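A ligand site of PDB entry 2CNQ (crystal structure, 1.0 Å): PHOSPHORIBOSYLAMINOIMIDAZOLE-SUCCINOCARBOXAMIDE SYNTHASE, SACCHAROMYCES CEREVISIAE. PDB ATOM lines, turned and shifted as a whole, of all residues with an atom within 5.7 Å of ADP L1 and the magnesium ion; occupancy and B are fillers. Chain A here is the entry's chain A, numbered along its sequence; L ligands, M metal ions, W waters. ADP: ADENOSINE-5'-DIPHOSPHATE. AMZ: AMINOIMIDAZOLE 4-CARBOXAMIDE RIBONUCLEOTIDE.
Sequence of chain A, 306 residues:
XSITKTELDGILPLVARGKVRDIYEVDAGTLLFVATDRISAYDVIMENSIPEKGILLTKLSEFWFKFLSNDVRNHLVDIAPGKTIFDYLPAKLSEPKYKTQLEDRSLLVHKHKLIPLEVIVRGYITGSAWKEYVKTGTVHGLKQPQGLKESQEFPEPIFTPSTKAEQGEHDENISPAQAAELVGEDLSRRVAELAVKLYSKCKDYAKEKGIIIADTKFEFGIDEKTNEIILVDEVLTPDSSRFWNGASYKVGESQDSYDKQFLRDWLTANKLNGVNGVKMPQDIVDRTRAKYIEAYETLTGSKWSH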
ATOM      1  N   ARG A  17       1.726  13.455   2.652  1.00  0.00           N
ATOM      2  CA  ARG A  17       2.617  14.291   1.901  1.00  0.00           C
ATOM      3  C   ARG A  17       3.584  14.891   2.855  1.00  0.00           C
ATOM      4  O   ARG A  17       3.200  15.547   3.814  1.00  0.00           O
ATOM      5  CB  ARG A  17       1.910  15.387   1.140  1.00  0.00           C
ATOM      6  CG  ARG A  17       1.093  14.892   0.020  1.00  0.00           C
ATOM      7  CD  ARG A  17       0.705  16.010  -0.903  1.00  0.00           C
ATOM      8  NE  ARG A  17       0.061  15.538  -2.104  1.00  0.00           N
ATOM      9  CZ  ARG A  17      -1.240  15.327  -2.236  1.00  0.00           C
ATOM     10  NH1 ARG A  17      -1.712  14.875  -3.357  1.00  0.00           N
ATOM     11  NH2 ARG A  17      -2.051  15.612  -1.255  1.00  0.00           N
ATOM     12  N   GLY A  18       4.852  14.673   2.598  1.00  0.00           N
ATOM     13  CA  GLY A  18       5.906  15.358   3.299  1.00  0.00           C
ATOM     14  C   GLY A  18       6.193  16.643   2.580  1.00  0.00           C
ATOM     15  O   GLY A  18       5.453  17.070   1.711  1.00  0.00           O
ATOM     16  N   LYS A  19       7.298  17.261   2.908  1.00  0.00           N
ATOM     17  CA  LYS A  19       7.649  18.459   2.224  1.00  0.00           C
ATOM     18  C   LYS A  19       7.937  18.190   0.771  1.00  0.00           C
ATOM     19  O   LYS A  19       7.732  19.049  -0.053  1.00  0.00           O
ATOM     20  CB  LYS A  19       8.749  19.173   2.934  1.00  0.00           C
ATOM     21  CG  LYS A  19       8.233  19.685   4.270  1.00  0.00           C
ATOM     22  CD  LYS A  19       9.275  20.430   5.044  1.00  0.00           C
ATOM     23  CE  LYS A  19      10.468  19.540   5.455  1.00  0.00           C
ATOM     24  NZ  LYS A  19      10.031  18.426   6.355  1.00  0.00           N
ATOM     25  N   VAL A  20       8.444  17.031   0.493  1.00  0.00           N
ATOM     26  CA  VAL A  20       8.862  16.696  -0.847  1.00  0.00           C
ATOM     27  C   VAL A  20       8.096  15.563  -1.434  1.00  0.00           C
ATOM     28  O   VAL A  20       7.831  15.561  -2.619  1.00  0.00           O
ATOM     29  CB  VAL A  20      10.366  16.370  -0.850  1.00  0.00           C
ATOM     30  CG1 VAL A  20      10.809  15.800  -2.168  1.00  0.00           C
ATOM     31  CG2 VAL A  20      11.134  17.627  -0.535  1.00  0.00           C
ATOM     32  N   ARG A  21       7.758  14.568  -0.649  1.00  0.00           N
ATOM     33  CA  ARG A  21       7.205  13.374  -1.182  1.00  0.00           C
ATOM     34  C   ARG A  21       5.734  13.282  -0.958  1.00  0.00           C
ATOM     35  O   ARG A  21       5.196  13.741   0.029  1.00  0.00           O
ATOM     36  CB  ARG A  21       7.882  12.188  -0.610  1.00  0.00           C
ATOM     37  CG  ARG A  21       9.323  12.211  -1.094  1.00  0.00           C
ATOM     38  CD  ARG A  21      10.235  11.445  -0.285  1.00  0.00           C
ATOM     39  NE  ARG A  21      11.510  11.447  -0.899  1.00  0.00           N
ATOM     40  CZ  ARG A  21      12.381  12.423  -0.836  1.00  0.00           C
ATOM     41  NH1 ARG A  21      12.298  13.370   0.065  1.00  0.00           N
ATOM     42  NH2 ARG A  21      13.398  12.391  -1.678  1.00  0.00           N
ATOM     43  N   ASP A  22       5.089  12.660  -1.912  1.00  0.00           N
ATOM     44  CA  ASP A  22       3.709  12.224  -1.818  1.00  0.00           C
ATOM     45  C   ASP A  22       3.776  10.739  -1.715  1.00  0.00           C
ATOM     46  O   ASP A  22       4.410  10.099  -2.538  1.00  0.00           O
ATOM     47  CB  ASP A  22       2.896  12.627  -3.025  1.00  0.00           C
ATOM     48  CG  ASP A  22       2.709  14.086  -3.172  1.00  0.00           C
ATOM     49  OD1 ASP A  22       1.953  14.467  -4.099  1.00  0.00           O
ATOM     50  OD2 ASP A  22       3.232  14.888  -2.399  1.00  0.00           O
ATOM     51  N   ILE A  23       3.149  10.200  -0.700  1.00  0.00           N
ATOM     52  CA  ILE A  23       3.344   8.815  -0.354  1.00  0.00           C
ATOM     53  C   ILE A  23       2.004   8.165  -0.356  1.00  0.00           C
ATOM     54  O   ILE A  23       1.121   8.589   0.376  1.00  0.00           O
ATOM     55  CB  ILE A  23       4.004   8.706   0.964  1.00  0.00           C
ATOM     56  CG1 ILE A  23       5.312   9.498   0.944  1.00  0.00           C
ATOM     57  CG2 ILE A  23       4.265   7.242   1.304  1.00  0.00           C
ATOM     58  CD1 ILE A  23       5.951   9.576   2.220  1.00  0.00           C
ATOM     59  N   LEU A  31       4.591   1.132  -0.184  1.00  0.00           N
ATOM     60  CA  LEU A  31       4.288   2.507  -0.460  1.00  0.00           C
ATOM     61  C   LEU A  31       4.792   2.860  -1.820  1.00  0.00           C
ATOM     62  O   LEU A  31       5.800   2.387  -2.277  1.00  0.00           O
ATOM     63  CB  LEU A  31       4.979   3.399   0.534  1.00  0.00           C
ATOM     64  CG  LEU A  31       4.629   3.146   1.964  1.00  0.00           C
ATOM     65  CD1 LEU A  31       5.593   3.946   2.821  1.00  0.00           C
ATOM     66  CD2 LEU A  31       3.212   3.495   2.266  1.00  0.00           C
ATOM     67  N   PHE A  33       6.322   5.968  -3.270  1.00  0.00           N
ATOM     68  CA  PHE A  33       7.066   7.004  -2.614  1.00  0.00           C
ATOM     69  C   PHE A  33       7.496   7.990  -3.693  1.00  0.00           C
ATOM     70  O   PHE A  33       8.445   7.729  -4.401  1.00  0.00           O
ATOM     71  CB  PHE A  33       8.256   6.275  -1.977  1.00  0.00           C
ATOM     72  CG  PHE A  33       9.028   7.060  -0.991  1.00  0.00           C
ATOM     73  CD1 PHE A  33      10.303   7.484  -1.271  1.00  0.00           C
ATOM     74  CD2 PHE A  33       8.524   7.293   0.236  1.00  0.00           C
ATOM     75  CE1 PHE A  33      11.050   8.113  -0.305  1.00  0.00           C
ATOM     76  CE2 PHE A  33       9.269   7.910   1.210  1.00  0.00           C
ATOM     77  CZ  PHE A  33      10.525   8.332   0.924  1.00  0.00           C
ATOM     78  N   ARG A  38       8.681  19.729  -5.235  1.00  0.00           N
ATOM     79  CA  ARG A  38       8.657  20.710  -4.212  1.00  0.00           C
ATOM     80  C   ARG A  38      10.036  20.841  -3.591  1.00  0.00           C
ATOM     81  O   ARG A  38      10.832  19.926  -3.566  1.00  0.00           O
ATOM     82  CB  ARG A  38       7.676  20.309  -3.119  1.00  0.00           C
ATOM     83  CG  ARG A  38       6.246  20.242  -3.614  1.00  0.00           C
ATOM     84  CD  ARG A  38       5.266  20.057  -2.518  1.00  0.00           C
ATOM     85  NE  ARG A  38       5.471  18.856  -1.745  1.00  0.00           N
ATOM     86  CZ  ARG A  38       4.795  17.733  -1.884  1.00  0.00           C
ATOM     87  NH1 ARG A  38       4.987  16.738  -1.061  1.00  0.00           N
ATOM     88  NH2 ARG A  38       3.934  17.588  -2.859  1.00  0.00           N
ATOM     89  N   HIS A  75      14.894   0.025   1.708  1.00  0.00           N
ATOM     90  CA  HIS A  75      13.468  -0.100   1.596  1.00  0.00           C
ATOM     91  C   HIS A  75      12.950  -0.357   0.224  1.00  0.00           C
ATOM     92  O   HIS A  75      11.757  -0.492   0.057  1.00  0.00           O
ATOM     93  CB  HIS A  75      12.760   1.111   2.164  1.00  0.00           C
ATOM     94  CG  HIS A  75      12.967   2.377   1.470  1.00  0.00           C
ATOM     95  ND1 HIS A  75      12.134   3.423   1.751  1.00  0.00           N
ATOM     96  CD2 HIS A  75      13.845   2.805   0.543  1.00  0.00           C
ATOM     97  CE1 HIS A  75      12.499   4.444   1.033  1.00  0.00           C
ATOM     98  NE2 HIS A  75      13.543   4.104   0.295  1.00  0.00           N
ATOM     99  N   VAL A 109       8.406   1.111  -2.262  1.00  0.00           N
ATOM    100  CA  VAL A 109       9.198   0.835  -1.109  1.00  0.00           C
ATOM    101  C   VAL A 109       8.378   0.070  -0.127  1.00  0.00           C
ATOM    102  O   VAL A 109       7.170   0.164  -0.059  1.00  0.00           O
ATOM    103  CB  VAL A 109       9.755   2.105  -0.462  1.00  0.00           C
ATOM    104  CG1 VAL A 109      10.555   2.894  -1.488  1.00  0.00           C
ATOM    105  CG2 VAL A 109       8.703   2.950   0.134  1.00  0.00           C
ATOM    106  N   HIS A 110       9.082  -0.681   0.662  1.00  0.00           N
ATOM    107  CA  HIS A 110       8.477  -1.341   1.755  1.00  0.00           C
ATOM    108  C   HIS A 110       8.253  -0.359   2.865  1.00  0.00           C
ATOM    109  O   HIS A 110       9.115   0.405   3.222  1.00  0.00           O
ATOM    110  CB  HIS A 110       9.456  -2.388   2.258  1.00  0.00           C
ATOM    111  CG  HIS A 110       9.675  -3.509   1.310  1.00  0.00           C
ATOM    112  ND1 HIS A 110       8.752  -4.507   1.130  1.00  0.00           N
ATOM    113  CD2 HIS A 110      10.719  -3.807   0.495  1.00  0.00           C
ATOM    114  CE1 HIS A 110       9.203  -5.356   0.237  1.00  0.00           C
ATOM    115  NE2 HIS A 110      10.412  -4.969  -0.147  1.00  0.00           N
ATOM    116  N   LYS A 111       7.074  -0.397   3.427  1.00  0.00           N
ATOM    117  CA  LYS A 111       6.781   0.365   4.608  1.00  0.00           C
ATOM    118  C   LYS A 111       7.633  -0.198   5.698  1.00  0.00           C
ATOM    119  O   LYS A 111       7.598  -1.375   5.952  1.00  0.00           O
ATOM    120  CB  LYS A 111       5.275   0.292   4.804  1.00  0.00           C
ATOM    121  CG  LYS A 111       4.745   1.170   5.882  1.00  0.00           C
ATOM    122  CD  LYS A 111       3.228   0.963   6.131  1.00  0.00           C
ATOM    123  CE  LYS A 111       2.290   0.743   4.881  1.00  0.00           C
ATOM    124  NZ  LYS A 111       0.768   0.351   5.122  1.00  0.00           N
ATOM    125  N   HIS A 112       8.375   0.627   6.384  1.00  0.00           N
ATOM    126  CA  HIS A 112       9.158   0.163   7.483  1.00  0.00           C
ATOM    127  C   HIS A 112       8.858   0.943   8.677  1.00  0.00           C
ATOM    128  O   HIS A 112       8.520   2.114   8.615  1.00  0.00           O
ATOM    129  CB  HIS A 112      10.640   0.267   7.190  1.00  0.00           C
ATOM    130  CG  HIS A 112      11.144  -0.889   6.420  1.00  0.00           C
ATOM    131  ND1 HIS A 112      11.245  -2.129   6.981  1.00  0.00           N
ATOM    132  CD2 HIS A 112      11.518  -1.023   5.130  1.00  0.00           C
ATOM    133  CE1 HIS A 112      11.687  -2.979   6.085  1.00  0.00           C
ATOM    134  NE2 HIS A 112      11.841  -2.345   4.952  1.00  0.00           N
ATOM    135  N   LEU A 114      10.160   3.096  11.251  1.00  0.00           N
ATOM    136  CA  LEU A 114      11.245   4.019  11.178  1.00  0.00           C
ATOM    137  C   LEU A 114      11.860   4.186  12.519  1.00  0.00           C
ATOM    138  O   LEU A 114      11.208   4.117  13.518  1.00  0.00           O
ATOM    139  CB  LEU A 114      10.789   5.380  10.670  1.00  0.00           C
ATOM    140  CG  LEU A 114      10.125   5.316   9.336  1.00  0.00           C
ATOM    141  CD1 LEU A 114       9.682   6.692   8.942  1.00  0.00           C
ATOM    142  CD2 LEU A 114      11.029   4.597   8.345  1.00  0.00           C
ATOM    143  N   LYS A 164      13.046  13.928  14.896  1.00  0.00           N
ATOM    144  CA  LYS A 164      12.117  14.156  13.818  1.00  0.00           C
ATOM    145  C   LYS A 164      10.995  14.961  14.384  1.00  0.00           C
ATOM    146  O   LYS A 164      10.161  14.424  15.131  1.00  0.00           O
ATOM    147  CB  LYS A 164      11.608  12.828  13.271  1.00  0.00           C
ATOM    148  CG  LYS A 164      12.705  12.038  12.646  1.00  0.00           C
ATOM    149  CD  LYS A 164      12.293  10.649  12.277  1.00  0.00           C
ATOM    150  CE  LYS A 164      11.344  10.654  11.157  1.00  0.00           C
ATOM    151  NZ  LYS A 164      10.945   9.293  10.893  1.00  0.00           N
ATOM    152  N   LYS A 217      21.989  13.507   6.058  1.00  0.00           N
ATOM    153  CA  LYS A 217      20.961  12.953   6.880  1.00  0.00           C
ATOM    154  C   LYS A 217      20.468  11.702   6.257  1.00  0.00           C
ATOM    155  O   LYS A 217      19.948  11.722   5.157  1.00  0.00           O
ATOM    156  CB  LYS A 217      19.839  13.956   7.028  1.00  0.00           C
ATOM    157  CG  LYS A 217      18.696  13.469   7.881  1.00  0.00           C
ATOM    158  CD  LYS A 217      17.633  12.678   7.187  1.00  0.00           C
ATOM    159  CE  LYS A 217      16.815  13.511   6.262  1.00  0.00           C
ATOM    160  NZ  LYS A 217      15.849  12.721   5.471  1.00  0.00           N
ATOM    161  N   GLU A 219      17.922   8.318   6.924  1.00  0.00           N
ATOM    162  CA  GLU A 219      16.869   7.768   7.696  1.00  0.00           C
ATOM    163  C   GLU A 219      16.979   6.301   7.666  1.00  0.00           C
ATOM    164  O   GLU A 219      17.261   5.697   6.644  1.00  0.00           O
ATOM    165  CB  GLU A 219      15.514   8.200   7.190  1.00  0.00           C
ATOM    166  CG  GLU A 219      15.328   9.673   7.282  1.00  0.00           C
ATOM    167  CD  GLU A 219      13.944  10.143   7.032  1.00  0.00           C
ATOM    168  OE1 GLU A 219      13.805  11.348   6.719  1.00  0.00           O
ATOM    169  OE2 GLU A 219      13.002   9.334   7.143  1.00  0.00           O
ATOM    170  N   VAL A 232      16.258   3.836   4.545  1.00  0.00           N
ATOM    171  CA  VAL A 232      14.980   4.218   3.989  1.00  0.00           C
ATOM    172  C   VAL A 232      15.068   5.615   3.435  1.00  0.00           C
ATOM    173  O   VAL A 232      16.127   6.177   3.266  1.00  0.00           O
ATOM    174  CB  VAL A 232      13.848   4.077   5.015  1.00  0.00           C
ATOM    175  CG1 VAL A 232      13.829   2.674   5.557  1.00  0.00           C
ATOM    176  CG2 VAL A 232      13.968   5.062   6.116  1.00  0.00           C
ATOM    177  N   ASP A 233      13.938   6.160   3.067  1.00  0.00           N
ATOM    178  CA  ASP A 233      13.845   7.523   2.652  1.00  0.00           C
ATOM    179  C   ASP A 233      14.716   7.778   1.440  1.00  0.00           C
ATOM    180  O   ASP A 233      14.681   6.987   0.513  1.00  0.00           O
ATOM    181  CB  ASP A 233      14.110   8.465   3.811  1.00  0.00           C
ATOM    182  CG  ASP A 233      13.615   9.839   3.571  1.00  0.00           C
ATOM    183  OD1 ASP A 233      12.383  10.014   3.553  1.00  0.00           O
ATOM    184  OD2 ASP A 233      14.460  10.738   3.428  1.00  0.00           O
ATOM    185  N   GLU A 234      15.360   8.908   1.421  1.00  0.00           N
ATOM    186  CA  GLU A 234      16.290   9.269   0.399  1.00  0.00           C
ATOM    187  C   GLU A 234      17.677   9.184   0.956  1.00  0.00           C
ATOM    188  O   GLU A 234      17.901   9.272   2.136  1.00  0.00           O
ATOM    189  CB  GLU A 234      16.005  10.647  -0.148  1.00  0.00           C
ATOM    190  CG  GLU A 234      16.373  11.741   0.809  1.00  0.00           C
ATOM    191  CD  GLU A 234      16.055  13.107   0.302  1.00  0.00           C
ATOM    192  OE1 GLU A 234      15.773  13.962   1.164  1.00  0.00           O
ATOM    193  OE2 GLU A 234      16.101  13.321  -0.911  1.00  0.00           O
HETATM  194  PB  ADP L   1       9.657  15.163   5.238  1.00  0.00           P
HETATM  195  O1B ADP L   1      11.098  15.190   5.002  1.00  0.00           O
HETATM  196  O2B ADP L   1       9.313  14.727   6.599  1.00  0.00           O
HETATM  197  O3B ADP L   1       8.900  16.372   4.956  1.00  0.00           O
HETATM  198  PA  ADP L   1       9.406  13.687   2.816  1.00  0.00           P
HETATM  199  O1A ADP L   1      10.856  13.485   2.673  1.00  0.00           O
HETATM  200  O2A ADP L   1       8.735  14.614   1.924  1.00  0.00           O
HETATM  201  O3A ADP L   1       9.055  14.033   4.297  1.00  0.00           O
HETATM  202  O5' ADP L   1       8.643  12.321   2.683  1.00  0.00           O
HETATM  203  C5' ADP L   1       9.141  11.066   3.088  1.00  0.00           C
HETATM  204  C4' ADP L   1       8.405  10.617   4.323  1.00  0.00           C
HETATM  205  O4' ADP L   1       8.362   9.199   4.256  1.00  0.00           O
HETATM  206  C3' ADP L   1       9.117  10.945   5.600  1.00  0.00           C
HETATM  207  O3' ADP L   1       8.193  11.002   6.658  1.00  0.00           O
HETATM  208  C2' ADP L   1       9.974   9.724   5.814  1.00  0.00           C
HETATM  209  O2' ADP L   1      10.400   9.562   7.122  1.00  0.00           O
HETATM  210  C1' ADP L   1       9.038   8.670   5.383  1.00  0.00           C
HETATM  211  N9  ADP L   1       9.613   7.421   4.968  1.00  0.00           N
HETATM  212  C8  ADP L   1      10.745   7.264   4.275  1.00  0.00           C
HETATM  213  N7  ADP L   1      10.968   6.006   3.961  1.00  0.00           N
HETATM  214  C5  ADP L   1       9.928   5.341   4.489  1.00  0.00           C
HETATM  215  C6  ADP L   1       9.533   3.981   4.494  1.00  0.00           C
HETATM  216  N6  ADP L   1      10.250   3.056   3.882  1.00  0.00           N
HETATM  217  N1  ADP L   1       8.460   3.624   5.183  1.00  0.00           N
HETATM  218  C2  ADP L   1       7.728   4.561   5.771  1.00  0.00           C
HETATM  219  N3  ADP L   1       7.950   5.868   5.764  1.00  0.00           N
HETATM  220  C4  ADP L   1       9.056   6.233   5.130  1.00  0.00           C
HETATM  221  O5  AMZ L   2      15.459  16.689   6.026  1.00  0.00           O
HETATM  222  C6  AMZ L   2      15.858  16.857   7.160  1.00  0.00           C
HETATM  223  N2  AMZ L   2      15.057  16.854   8.223  1.00  0.00           N
HETATM  224  C3A AMZ L   2      17.263  17.068   7.421  1.00  0.00           C
HETATM  225  C7A AMZ L   2      18.243  17.157   6.486  1.00  0.00           C
HETATM  226  N3  AMZ L   2      18.241  17.011   5.150  1.00  0.00           N
HETATM  227  N1  AMZ L   2      17.801  17.249   8.644  1.00  0.00           N
HETATM  228  C5  AMZ L   2      19.081  17.431   8.475  1.00  0.00           C
HETATM  229  N   AMZ L   2      19.380  17.391   7.150  1.00  0.00           N
HETATM  230  C1  AMZ L   2      20.693  17.486   6.577  1.00  0.00           C
HETATM  231  C2  AMZ L   2      21.076  18.852   6.109  1.00  0.00           C
HETATM  232  C3  AMZ L   2      22.563  18.835   6.220  1.00  0.00           C
HETATM  233  O2  AMZ L   2      23.044  18.152   5.083  1.00  0.00           O
HETATM  234  O1  AMZ L   2      20.584  19.055   4.789  1.00  0.00           O
HETATM  235  O   AMZ L   2      21.588  17.205   7.622  1.00  0.00           O
HETATM  236  C   AMZ L   2      22.773  17.984   7.464  1.00  0.00           C
HETATM  237  C4  AMZ L   2      23.041  18.770   8.709  1.00  0.00           C
HETATM  238  O3  AMZ L   2      22.122  19.845   8.765  1.00  0.00           O
HETATM  239  P   AMZ L   2      22.320  20.942   9.903  1.00  0.00           P
HETATM  240  OP1 AMZ L   2      21.950  20.304  11.203  1.00  0.00           O
HETATM  241  O4  AMZ L   2      21.359  22.037   9.512  1.00  0.00           O
HETATM  242  OP2 AMZ L   2      23.746  21.401   9.914  1.00  0.00           O
HETATM  243 MG    MG M   1      12.355  14.150   3.915  1.00  0.00          MG
HETATM  244  O   HOH W   1      13.781  13.187   2.930  1.00  0.00           O
HETATM  245  O   HOH W   2       6.696  17.011   6.505  1.00  0.00           O
HETATM  246  O   HOH W   3      12.120  12.362   4.896  1.00  0.00           O
HETATM  247  O   HOH W   4       5.515  10.061   6.323  1.00  0.00           O
HETATM  248  O   HOH W   5      12.825  15.757   2.788  1.00  0.00           O
HETATM  249  O   HOH W   6       9.347  16.477   8.648  1.00  0.00           O
HETATM  250  O   HOH W   7      13.759  14.678   5.398  1.00  0.00           O
HETATM  251  O   HOH W   8       6.293   6.356   7.956  1.00  0.00           O
HETATM  252  O   HOH W   9       5.247   7.625   4.976  1.00  0.00           O
HETATM  253  O   HOH W  10       7.074  13.435   7.141  1.00  0.00           O
HETATM  254  O   HOH W  11      10.029  12.917   8.142  1.00  0.00           O
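An oxygen (O3B) of ADP L1 sits at hydrogen-bond distance from the backbone NH of Lys 19.
N of Arg 21 sits at hydrogen-bond distance from O2A of ADP L1 (2.8 Å).
The side-chain amino group of Lys 19 lies within salt-bridge range of an oxygen (O3B) of ADP L1, 2.7 Å away.
A ring nitrogen (ND1) of His 75 sits at hydrogen-bond distance from a nitrogen (N6) of ADP L1 (2.9 Å).
The backbone NH (N) of Asp 233 is in hydrogen-bond range of a nitrogen (N7) of ADP L1 (3.1 Å).
The side-chain carboxylate (OE2) of Glu 219 sits at hydrogen-bond distance from an oxygen (O2') of ADP L1 (2.6 Å).
An oxygen (O1A) of ADP L1 sits close to the guanidinium group (NH1) of Arg 21 (3.0 Å).
The backbone NH (N) of Val 20 is in hydrogen-bond range of an oxygen (O2A) of ADP L1, at 2.8 Å.
A nitrogen (N1) of ADP L1 sits at hydrogen-bond distance from the backbone NH of His 112.
The backbone carbonyl oxygen (O) of His 110 is in hydrogen-bond range of a nitrogen (N6) of ADP L1, 3.0 Å away.
The backbone carbonyl oxygen (O) of Asp 233 is in hydrogen-bond range of a ring nitrogen (NE2) of His 75, at 3.1 Å.
The side-chain carboxylate (OD2) of Asp 233 lies within salt-bridge range of the side-chain amino group (NZ) of Lys 217, at 3.2 Å.
The backbone NH (N) of Leu 31 lies within hydrogen-bond range of the backbone carbonyl oxygen (O) of Val 109, 2.8 Å away.
The backbone carbonyl oxygen of Gly 18 lies within hydrogen-bond range of the guanidinium group of Arg 38 (2.8 Å).
The backbone carbonyl oxygen (O) of Arg 21 is in hydrogen-bond range of the guanidinium group (NH1) of Arg 38.
O of Lys 19 lies within hydrogen-bond range of NE of Arg 38, at 2.8 Å.
The backbone carbonyl oxygen (O) of Val 20 sits close to the guanidinium group (NH1) of Arg 38.
The backbone NH (N) of His 110 lies within hydrogen-bond range of the backbone carbonyl oxygen (O) of His 75, 2.7 Å away.
Gly 18 touches ADP L1 (CA to O2A, 3.2 Å).
CD1 of Ile 23 touches O4' of ADP L1 (3.2 Å).
CD1 of Leu 31 touches C2 of ADP L1, at 3.7 Å.
Phe 33 touches ADP L1.
CA of Lys 111 touches N1 of ADP L1 (3.7 Å).
Leu 114 touches ADP L1 (CD1 to O2', 3.5 Å).
Lys 164 touches ADP L1 (NZ to O2', 3.8 Å).
Val 232 touches ADP L1 (CB to N7, 3.6 Å).
16 residues have an atom within 4 Å of ADP L1: Gly 18, Lys 19, Val 20, Arg 21, Ile 23, Leu 31, Phe 33, His 75, His 110, Lys 111, His 112, Leu 114, Lys 164, Glu 219, Val 232 and Asp 233.
Residues that only touch the magnesium ion: Arg 21 (3.9 Å).
Of the 22 residues printed, 1 comes within 4 Å of the magnesium ion.
The nearest printed residue that does not touch the magnesium ion is Asp 233 (4.04 Å).
The magnesium ion is bound by an oxygen (O1B) of ADP L1 (2.0 Å), water W1 (2.0 Å), water W5 (2.0 Å), water W3 (2.1 Å), an oxygen (O1A) of ADP L1 (2.1 Å) and water W7 (2.1 Å).
The magnesium ion has six donor atoms within binding distance.
Water W1 lies within hydrogen-bond range of the side-chain carboxylate (OD2) of Asp 233 (2.6 Å), the side-chain carboxylate (OE1) of Glu 234 (2.8 Å), the guanidinium group (NH1) of Arg 21 (3.2 Å) and the side-chain amino group (NZ) of Lys 217 (3.3 Å).
Water W7 bridges an oxygen (O5) of AMZ L2 (2.7 Å) and the side-chain amino group of Lys 217 (2.9 Å).
Water W3 lies within hydrogen-bond range of OE1 of Glu 219 (2.7 Å) and OD1 of Asp 233 (2.7 Å).
Water W6 lies within hydrogen-bond range of an oxygen (O2B) of ADP L1 (2.7 Å) and the side-chain amino group of Lys 19 (3.1 Å).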
